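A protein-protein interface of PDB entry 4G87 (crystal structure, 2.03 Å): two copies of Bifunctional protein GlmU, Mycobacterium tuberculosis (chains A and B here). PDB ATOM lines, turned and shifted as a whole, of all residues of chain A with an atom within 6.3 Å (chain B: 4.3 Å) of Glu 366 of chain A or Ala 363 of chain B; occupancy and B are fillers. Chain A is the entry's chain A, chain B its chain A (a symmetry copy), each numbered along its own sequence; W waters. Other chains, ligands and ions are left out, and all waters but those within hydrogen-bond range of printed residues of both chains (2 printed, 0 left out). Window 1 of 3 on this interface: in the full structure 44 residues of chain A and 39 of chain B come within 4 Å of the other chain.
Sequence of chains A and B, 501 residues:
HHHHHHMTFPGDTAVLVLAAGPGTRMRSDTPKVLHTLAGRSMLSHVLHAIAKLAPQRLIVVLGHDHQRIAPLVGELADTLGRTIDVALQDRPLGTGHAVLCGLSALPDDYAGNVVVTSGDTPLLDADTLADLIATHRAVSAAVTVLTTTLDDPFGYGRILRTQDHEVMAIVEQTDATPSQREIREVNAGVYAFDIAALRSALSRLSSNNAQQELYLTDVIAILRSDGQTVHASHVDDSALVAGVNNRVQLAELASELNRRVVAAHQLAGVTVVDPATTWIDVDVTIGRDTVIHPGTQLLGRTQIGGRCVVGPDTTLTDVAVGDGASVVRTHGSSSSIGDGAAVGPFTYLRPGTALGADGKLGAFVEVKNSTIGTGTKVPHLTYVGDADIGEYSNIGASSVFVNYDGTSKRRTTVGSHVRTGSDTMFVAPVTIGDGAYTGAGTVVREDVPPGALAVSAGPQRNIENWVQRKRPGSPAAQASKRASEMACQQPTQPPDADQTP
The backbone NH (N) of Tyr 348 of chain A sits at hydrogen-bond distance from the backbone carbonyl oxygen (O) of Val 365 of chain A. The guanidinium group of Arg 350 of chain A is in salt-bridge range of the side-chain carboxylate of Glu 366 of chain A (2.8 Å). O of Thr 382 of chain A sits at hydrogen-bond distance from N of Glu 366 of chain A, 3.0 Å away. O of Ala 363 of chain B is in hydrogen-bond range of N of Leu 381 of chain B, at 3.1 Å. The backbone carbonyl oxygen (O) of Phe 346 of chain B sits at hydrogen-bond distance from the backbone NH (N) of Phe 364 of chain B, 2.7 Å away. The side-chain hydroxyl (OG1) of Thr 347 of chain A sits at hydrogen-bond distance from the backbone carbonyl oxygen (O) of Gly 362 of chain A (2.7 Å).
The side-chain carboxylate (OE1) of Glu 366 of chain A is in hydrogen-bond range of a ring nitrogen (ND1) of His 380 of chain B (2.9 Å).
Of the printed residues of chain B, Phe 346 of chain A touches Phe 346 and Phe 364. Printed residues of chain B within 4 Å of Thr 347 of chain A: Phe 346 (3.6 Å). Printed residues of chain B within 4 Å of Tyr 348 of chain A: Pro 345 and Ala 363. Gly 362 of chain A touches none of the printed residues of chain B. Of chain B, only Ala 363 (3.6 Å), Phe 364 (3.9 Å) and His 380 (2.9 Å) come within 4 Å of Glu 366 of chain A. Of the printed residues of chain B, Tyr 383 of chain A touches His 380 (3.3 Å) and Leu 381 (3.6 Å). Ala 363 of chain B touches just these residues of chain A: Tyr 348 and Glu 366. Pro 379 of chain B touches none of the printed residues of chain A. Printed residues of chain A within 4 Å of His 380 of chain B: Glu 366 and Tyr 383. The nearest printed residue of chain B that does not touch Glu 366 of chain A is Pro 379 of chain B (4.3 Å).
Hydrophobic or aromatic side chains of chain A that line the printed part of chain B: Tyr 348, Phe 364 and Tyr 383. Of the 9 printed residues of chain B, 6 touch a printed residue of chain A. Printed residues of chain B that touch a printed residue of chain A: Pro 345, Phe 346, Ala 363, Phe 364, His 380 and Leu 381. Hydrophobic or aromatic side chains of chain B that line the printed part of chain A: Pro 345, Phe 346, Ala 363, Phe 364, His 380 and Leu 381. Among the printed residues, no Asp or Glu carboxylate lies within 4 Å of a Lys or Arg side-chain nitrogen of the other chain.
CE1 of Phe 346 of chain B touches CA of Phe 346 of chain A (3.9 Å). Phe 346 of chain A touches Phe 364 of chain B (O to CZ, 3.3 Å). O of Thr 347 of chain A touches CE2 of Phe 346 of chain B, at 3.6 Å. CD of Pro 345 of chain B touches CE2 of Tyr 348 of chain A, at 3.5 Å. Phe 364 of chain A touches Phe 364 of chain B (C to CE2, 3.4 Å). CD2 of Leu 381 of chain B touches O of Phe 364 of chain A, 3.4 Å away. Ala 363 of chain B touches Glu 366 of chain A (CB to OE1, 3.6 Å). Thr 382 of chain A touches Leu 381 of chain B (C to CD1, 3.6 Å). Tyr 383 of chain A touches His 380 of chain B. Leu 381 of chain B touches Tyr 383 of chain A (CD1 to N, 3.6 Å).
Phe 346 of chain A touches its own counterpart, Phe 346 of chain B. Phe 346 of chain A touches Phe 364 of chain B, but with the chains exchanged Phe 364 of chain A does not touch Phe 346 of chain B (6.2 Å). Phe 364 of chain B touches its own counterpart, Phe 364 of chain A. Val 365 of chain A touches Phe 364 of chain B, but with the chains exchanged Phe 364 of chain A does not touch Val 365 of chain B (8.1 Å).
Water W1 lies within hydrogen-bond range of the side-chain carboxylate of Glu 366 of chain A (2.7 Å), the backbone carbonyl oxygen of Pro 379 of chain B (2.7 Å) and the backbone NH of Ala 363 of chain B (2.9 Å). Water W2 lies within hydrogen-bond range of O of Ala 363 of chain B (2.8 Å), OE1 of Glu 366 of chain A (2.8 Å) and ND1 of His 380 of chain B (3.1 Å).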
ATOM      1  N   PHE A 346      -2.935 -12.992 -16.039  1.00  0.00           N
ATOM      2  CA  PHE A 346      -1.810 -12.950 -15.061  1.00  0.00           C
ATOM      3  C   PHE A 346      -1.382 -11.517 -14.717  1.00  0.00           C
ATOM      4  O   PHE A 346      -0.220 -11.097 -14.942  1.00  0.00           O
ATOM      5  CB  PHE A 346      -0.577 -13.787 -15.432  1.00  0.00           C
ATOM      6  CG  PHE A 346      -0.884 -15.168 -16.011  1.00  0.00           C
ATOM      7  CD1 PHE A 346      -1.204 -16.264 -15.184  1.00  0.00           C
ATOM      8  CD2 PHE A 346      -0.772 -15.365 -17.382  1.00  0.00           C
ATOM      9  CE1 PHE A 346      -1.480 -17.585 -15.759  1.00  0.00           C
ATOM     10  CE2 PHE A 346      -1.007 -16.667 -17.959  1.00  0.00           C
ATOM     11  CZ  PHE A 346      -1.330 -17.753 -17.163  1.00  0.00           C
ATOM     12  N   THR A 347      -2.322 -10.795 -14.140  1.00  0.00           N
ATOM     13  CA  THR A 347      -2.109  -9.376 -13.798  1.00  0.00           C
ATOM     14  C   THR A 347      -2.472  -9.201 -12.330  1.00  0.00           C
ATOM     15  O   THR A 347      -3.480  -9.754 -11.873  1.00  0.00           O
ATOM     16  CB  THR A 347      -3.008  -8.476 -14.725  1.00  0.00           C
ATOM     17  OG1 THR A 347      -2.661  -8.788 -16.098  1.00  0.00           O
ATOM     18  CG2 THR A 347      -2.681  -6.975 -14.505  1.00  0.00           C
ATOM     19  N   TYR A 348      -1.648  -8.463 -11.588  1.00  0.00           N
ATOM     20  CA  TYR A 348      -1.894  -8.242 -10.148  1.00  0.00           C
ATOM     21  C   TYR A 348      -2.174  -6.737  -9.978  1.00  0.00           C
ATOM     22  O   TYR A 348      -1.299  -5.896 -10.360  1.00  0.00           O
ATOM     23  CB  TYR A 348      -0.598  -8.576  -9.376  1.00  0.00           C
ATOM     24  CG  TYR A 348      -0.607  -8.437  -7.866  1.00  0.00           C
ATOM     25  CD1 TYR A 348      -1.801  -8.464  -7.131  1.00  0.00           C
ATOM     26  CD2 TYR A 348       0.589  -8.335  -7.178  1.00  0.00           C
ATOM     27  CE1 TYR A 348      -1.777  -8.376  -5.742  1.00  0.00           C
ATOM     28  CE2 TYR A 348       0.617  -8.222  -5.794  1.00  0.00           C
ATOM     29  CZ  TYR A 348      -0.550  -8.267  -5.114  1.00  0.00           C
ATOM     30  OH  TYR A 348      -0.496  -8.193  -3.758  1.00  0.00           O
ATOM     31  N   LEU A 349      -3.359  -6.379  -9.470  1.00  0.00           N
ATOM     32  CA  LEU A 349      -3.661  -4.988  -9.138  1.00  0.00           C
ATOM     33  C   LEU A 349      -3.713  -4.802  -7.633  1.00  0.00           C
ATOM     34  O   LEU A 349      -4.456  -5.468  -6.947  1.00  0.00           O
ATOM     35  CB  LEU A 349      -5.028  -4.530  -9.714  1.00  0.00           C
ATOM     36  CG  LEU A 349      -5.225  -4.899 -11.182  1.00  0.00           C
ATOM     37  CD1 LEU A 349      -6.599  -4.378 -11.654  1.00  0.00           C
ATOM     38  CD2 LEU A 349      -4.097  -4.362 -12.080  1.00  0.00           C
ATOM     39  N   ARG A 350      -2.829  -3.974  -7.133  1.00  0.00           N
ATOM     40  CA  ARG A 350      -2.781  -3.596  -5.713  1.00  0.00           C
ATOM     41  C   ARG A 350      -3.528  -2.287  -5.446  1.00  0.00           C
ATOM     42  O   ARG A 350      -3.811  -1.543  -6.380  1.00  0.00           O
ATOM     43  CB  ARG A 350      -1.314  -3.486  -5.234  1.00  0.00           C
ATOM     44  CG  ARG A 350      -0.714  -4.889  -5.075  1.00  0.00           C
ATOM     45  CD  ARG A 350       0.791  -4.803  -4.937  1.00  0.00           C
ATOM     46  NE  ARG A 350       1.232  -4.184  -3.722  1.00  0.00           N
ATOM     47  CZ  ARG A 350       2.418  -3.578  -3.581  1.00  0.00           C
ATOM     48  NH1 ARG A 350       3.296  -3.473  -4.603  1.00  0.00           N
ATOM     49  NH2 ARG A 350       2.705  -3.039  -2.420  1.00  0.00           N
ATOM     50  N   GLY A 362      -1.269  -5.957 -19.205  1.00  0.00           N
ATOM     51  CA  GLY A 362      -1.098  -7.287 -19.820  1.00  0.00           C
ATOM     52  C   GLY A 362      -0.470  -8.316 -18.895  1.00  0.00           C
ATOM     53  O   GLY A 362      -0.531  -8.165 -17.658  1.00  0.00           O
ATOM     54  N   PHE A 364       1.795 -10.609 -16.671  1.00  0.00           N
ATOM     55  CA  PHE A 364       2.929 -10.466 -15.753  1.00  0.00           C
ATOM     56  C   PHE A 364       3.220  -8.971 -15.459  1.00  0.00           C
ATOM     57  O   PHE A 364       4.366  -8.540 -15.399  1.00  0.00           O
ATOM     58  CB  PHE A 364       4.168 -11.221 -16.278  1.00  0.00           C
ATOM     59  CG  PHE A 364       3.799 -12.519 -16.958  1.00  0.00           C
ATOM     60  CD1 PHE A 364       3.045 -13.482 -16.265  1.00  0.00           C
ATOM     61  CD2 PHE A 364       4.177 -12.733 -18.307  1.00  0.00           C
ATOM     62  CE1 PHE A 364       2.657 -14.674 -16.889  1.00  0.00           C
ATOM     63  CE2 PHE A 364       3.773 -13.880 -18.973  1.00  0.00           C
ATOM     64  CZ  PHE A 364       3.002 -14.856 -18.265  1.00  0.00           C
ATOM     65  N   VAL A 365       2.144  -8.220 -15.321  1.00  0.00           N
ATOM     66  CA  VAL A 365       2.185  -6.822 -14.975  1.00  0.00           C
ATOM     67  C   VAL A 365       1.552  -6.684 -13.584  1.00  0.00           C
ATOM     68  O   VAL A 365       0.547  -7.345 -13.277  1.00  0.00           O
ATOM     69  CB  VAL A 365       1.436  -5.956 -16.029  1.00  0.00           C
ATOM     70  CG1 VAL A 365       1.181  -4.459 -15.510  1.00  0.00           C
ATOM     71  CG2 VAL A 365       2.249  -6.049 -17.427  1.00  0.00           C
ATOM     72  N   GLU A 366       2.195  -5.892 -12.734  1.00  0.00           N
ATOM     73  CA  GLU A 366       1.625  -5.577 -11.414  1.00  0.00           C
ATOM     74  C   GLU A 366       1.580  -4.053 -11.363  1.00  0.00           C
ATOM     75  O   GLU A 366       2.544  -3.388 -11.801  1.00  0.00           O
ATOM     76  CB  GLU A 366       2.642  -6.041 -10.319  1.00  0.00           C
ATOM     77  CG  GLU A 366       2.320  -5.450  -8.955  1.00  0.00           C
ATOM     78  CD  GLU A 366       3.212  -5.986  -7.799  1.00  0.00           C
ATOM     79  OE1 GLU A 366       3.798  -7.103  -7.938  1.00  0.00           O
ATOM     80  OE2 GLU A 366       3.283  -5.289  -6.749  1.00  0.00           O
ATOM     81  N   VAL A 367       0.523  -3.490 -10.809  1.00  0.00           N
ATOM     82  CA  VAL A 367       0.397  -1.997 -10.618  1.00  0.00           C
ATOM     83  C   VAL A 367      -0.048  -1.812  -9.186  1.00  0.00           C
ATOM     84  O   VAL A 367      -0.810  -2.639  -8.671  1.00  0.00           O
ATOM     85  CB  VAL A 367      -0.660  -1.403 -11.580  1.00  0.00           C
ATOM     86  CG1 VAL A 367      -0.848   0.133 -11.349  1.00  0.00           C
ATOM     87  CG2 VAL A 367      -0.255  -1.749 -13.050  1.00  0.00           C
ATOM     88  N   LYS A 368       0.470  -0.763  -8.532  1.00  0.00           N
ATOM     89  CA  LYS A 368       0.189  -0.422  -7.141  1.00  0.00           C
ATOM     90  C   LYS A 368       0.120   1.122  -7.118  1.00  0.00           C
ATOM     91  O   LYS A 368       1.040   1.822  -7.667  1.00  0.00           O
ATOM     92  CB  LYS A 368       1.342  -0.885  -6.220  1.00  0.00           C
ATOM     93  CG  LYS A 368       1.230  -0.383  -4.729  1.00  0.00           C
ATOM     94  CD  LYS A 368       2.465   0.506  -4.374  1.00  0.00           C
ATOM     95  CE  LYS A 368       2.448   1.126  -2.971  1.00  0.00           C
ATOM     96  NZ  LYS A 368       3.900   1.686  -2.770  1.00  0.00           N
ATOM     97  N   THR A 382       5.948  -5.996 -16.404  1.00  0.00           N
ATOM     98  CA  THR A 382       6.323  -4.674 -15.845  1.00  0.00           C
ATOM     99  C   THR A 382       5.674  -4.356 -14.478  1.00  0.00           C
ATOM    100  O   THR A 382       4.547  -4.762 -14.190  1.00  0.00           O
ATOM    101  CB  THR A 382       6.389  -3.501 -16.908  1.00  0.00           C
ATOM    102  OG1 THR A 382       5.716  -2.260 -16.567  1.00  0.00           O
ATOM    103  CG2 THR A 382       6.463  -3.851 -18.277  1.00  0.00           C
ATOM    104  N   TYR A 383       6.441  -3.672 -13.658  1.00  0.00           N
ATOM    105  CA  TYR A 383       5.943  -3.181 -12.373  1.00  0.00           C
ATOM    106  C   TYR A 383       5.762  -1.659 -12.460  1.00  0.00           C
ATOM    107  O   TYR A 383       6.724  -0.928 -12.821  1.00  0.00           O
ATOM    108  CB  TYR A 383       6.895  -3.578 -11.235  1.00  0.00           C
ATOM    109  CG  TYR A 383       6.477  -2.910  -9.960  1.00  0.00           C
ATOM    110  CD1 TYR A 383       5.336  -3.330  -9.308  1.00  0.00           C
ATOM    111  CD2 TYR A 383       7.203  -1.796  -9.445  1.00  0.00           C
ATOM    112  CE1 TYR A 383       4.894  -2.666  -8.146  1.00  0.00           C
ATOM    113  CE2 TYR A 383       6.771  -1.127  -8.289  1.00  0.00           C
ATOM    114  CZ  TYR A 383       5.594  -1.601  -7.653  1.00  0.00           C
ATOM    115  OH  TYR A 383       5.135  -1.025  -6.504  1.00  0.00           O
ATOM    116  N   VAL A 384       4.536  -1.215 -12.206  1.00  0.00           N
ATOM    117  CA  VAL A 384       4.199   0.199 -12.121  1.00  0.00           C
ATOM    118  C   VAL A 384       3.796   0.534 -10.697  1.00  0.00           C
ATOM    119  O   VAL A 384       2.715   0.121 -10.254  1.00  0.00           O
ATOM    120  CB  VAL A 384       3.045   0.630 -13.107  1.00  0.00           C
ATOM    121  CG1 VAL A 384       2.911   2.171 -13.107  1.00  0.00           C
ATOM    122  CG2 VAL A 384       3.298   0.068 -14.568  1.00  0.00           C
ATOM    123  N   GLY A 385       4.639   1.294  -9.977  1.00  0.00           N
ATOM    124  CA  GLY A 385       4.305   1.651  -8.605  1.00  0.00           C
ATOM    125  C   GLY A 385       4.386   3.153  -8.420  1.00  0.00           C
ATOM    126  O   GLY A 385       5.349   3.775  -8.885  1.00  0.00           O
ATOM    127  N   PRO B 345       0.799 -13.012  -5.146  1.00  0.00           N
ATOM    128  CA  PRO B 345       0.200 -13.971  -6.053  1.00  0.00           C
ATOM    129  C   PRO B 345       1.093 -14.198  -7.290  1.00  0.00           C
ATOM    130  O   PRO B 345       1.928 -13.364  -7.622  1.00  0.00           O
ATOM    131  CB  PRO B 345      -1.131 -13.310  -6.447  1.00  0.00           C
ATOM    132  CG  PRO B 345      -0.686 -11.812  -6.546  1.00  0.00           C
ATOM    133  CD  PRO B 345       0.292 -11.651  -5.335  1.00  0.00           C
ATOM    134  N   PHE B 346       0.934 -15.345  -7.944  1.00  0.00           N
ATOM    135  CA  PHE B 346       1.695 -15.720  -9.169  1.00  0.00           C
ATOM    136  C   PHE B 346       3.186 -15.947  -8.890  1.00  0.00           C
ATOM    137  O   PHE B 346       4.080 -15.263  -9.446  1.00  0.00           O
ATOM    138  CB  PHE B 346       1.528 -14.776 -10.368  1.00  0.00           C
ATOM    139  CG  PHE B 346       0.100 -14.289 -10.614  1.00  0.00           C
ATOM    140  CD1 PHE B 346      -0.849 -15.084 -11.288  1.00  0.00           C
ATOM    141  CD2 PHE B 346      -0.249 -13.000 -10.228  1.00  0.00           C
ATOM    142  CE1 PHE B 346      -2.210 -14.591 -11.526  1.00  0.00           C
ATOM    143  CE2 PHE B 346      -1.574 -12.489 -10.487  1.00  0.00           C
ATOM    144  CZ  PHE B 346      -2.521 -13.258 -11.140  1.00  0.00           C
ATOM    145  N   GLY B 362       7.203 -12.324  -4.221  1.00  0.00           N
ATOM    146  CA  GLY B 362       6.049 -11.597  -4.782  1.00  0.00           C
ATOM    147  C   GLY B 362       5.643 -12.063  -6.170  1.00  0.00           C
ATOM    148  O   GLY B 362       5.955 -13.205  -6.561  1.00  0.00           O
ATOM    149  N   ALA B 363       4.907 -11.210  -6.895  1.00  0.00           N
ATOM    150  CA  ALA B 363       4.283 -11.627  -8.108  1.00  0.00           C
ATOM    151  C   ALA B 363       5.310 -11.774  -9.219  1.00  0.00           C
ATOM    152  O   ALA B 363       6.157 -10.882  -9.411  1.00  0.00           O
ATOM    153  CB  ALA B 363       3.211 -10.596  -8.510  1.00  0.00           C
ATOM    154  N   PHE B 364       5.194 -12.862  -9.976  1.00  0.00           N
ATOM    155  CA  PHE B 364       6.036 -13.188 -11.131  1.00  0.00           C
ATOM    156  C   PHE B 364       7.504 -13.437 -10.696  1.00  0.00           C
ATOM    157  O   PHE B 364       8.448 -13.013 -11.354  1.00  0.00           O
ATOM    158  CB  PHE B 364       5.916 -12.109 -12.229  1.00  0.00           C
ATOM    159  CG  PHE B 364       4.509 -11.566 -12.343  1.00  0.00           C
ATOM    160  CD1 PHE B 364       3.436 -12.445 -12.568  1.00  0.00           C
ATOM    161  CD2 PHE B 364       4.282 -10.178 -12.172  1.00  0.00           C
ATOM    162  CE1 PHE B 364       2.121 -11.968 -12.636  1.00  0.00           C
ATOM    163  CE2 PHE B 364       2.990  -9.675 -12.188  1.00  0.00           C
ATOM    164  CZ  PHE B 364       1.899 -10.573 -12.413  1.00  0.00           C
ATOM    165  N   VAL B 365       7.635 -14.097  -9.561  1.00  0.00           N
ATOM    166  CA  VAL B 365       8.906 -14.496  -9.012  1.00  0.00           C
ATOM    167  C   VAL B 365       8.950 -16.029  -9.048  1.00  0.00           C
ATOM    168  O   VAL B 365       7.943 -16.698  -8.768  1.00  0.00           O
ATOM    169  CB  VAL B 365       9.091 -13.956  -7.565  1.00  0.00           C
ATOM    170  CG1 VAL B 365      10.329 -14.648  -6.815  1.00  0.00           C
ATOM    171  CG2 VAL B 365       9.172 -12.340  -7.637  1.00  0.00           C
ATOM    172  N   PRO B 379      10.340  -9.056  -4.257  1.00  0.00           N
ATOM    173  CA  PRO B 379       8.942  -8.741  -4.539  1.00  0.00           C
ATOM    174  C   PRO B 379       8.441  -8.799  -5.984  1.00  0.00           C
ATOM    175  O   PRO B 379       7.222  -8.892  -6.164  1.00  0.00           O
ATOM    176  CB  PRO B 379       8.810  -7.301  -3.993  1.00  0.00           C
ATOM    177  CG  PRO B 379      10.215  -6.722  -4.286  1.00  0.00           C
ATOM    178  CD  PRO B 379      11.101  -7.862  -3.838  1.00  0.00           C
ATOM    179  N   HIS B 380       9.316  -8.718  -7.011  1.00  0.00           N
ATOM    180  CA  HIS B 380       8.792  -8.558  -8.369  1.00  0.00           C
ATOM    181  C   HIS B 380       9.623  -9.144  -9.480  1.00  0.00           C
ATOM    182  O   HIS B 380      10.826  -8.866  -9.560  1.00  0.00           O
ATOM    183  CB  HIS B 380       8.647  -7.085  -8.753  1.00  0.00           C
ATOM    184  CG  HIS B 380       7.950  -6.223  -7.731  1.00  0.00           C
ATOM    185  ND1 HIS B 380       6.587  -6.234  -7.567  1.00  0.00           N
ATOM    186  CD2 HIS B 380       8.425  -5.266  -6.881  1.00  0.00           C
ATOM    187  CE1 HIS B 380       6.249  -5.331  -6.646  1.00  0.00           C
ATOM    188  NE2 HIS B 380       7.345  -4.726  -6.228  1.00  0.00           N
ATOM    189  N   LEU B 381       8.973  -9.916 -10.353  1.00  0.00           N
ATOM    190  CA  LEU B 381       9.505 -10.207 -11.726  1.00  0.00           C
ATOM    191  C   LEU B 381      10.969 -10.659 -11.654  1.00  0.00           C
ATOM    192  O   LEU B 381      11.850 -10.200 -12.416  1.00  0.00           O
ATOM    193  CB  LEU B 381       9.374  -8.924 -12.574  1.00  0.00           C
ATOM    194  CG  LEU B 381       7.923  -8.523 -12.921  1.00  0.00           C
ATOM    195  CD1 LEU B 381       7.726  -6.998 -13.154  1.00  0.00           C
ATOM    196  CD2 LEU B 381       7.485  -9.326 -14.165  1.00  0.00           C
HETATM  197  O   HOH W   1       4.572  -8.519  -5.829  1.00  0.00           O
HETATM  198  O   HOH W   2       5.671  -8.111  -9.832  1.00  0.00           O
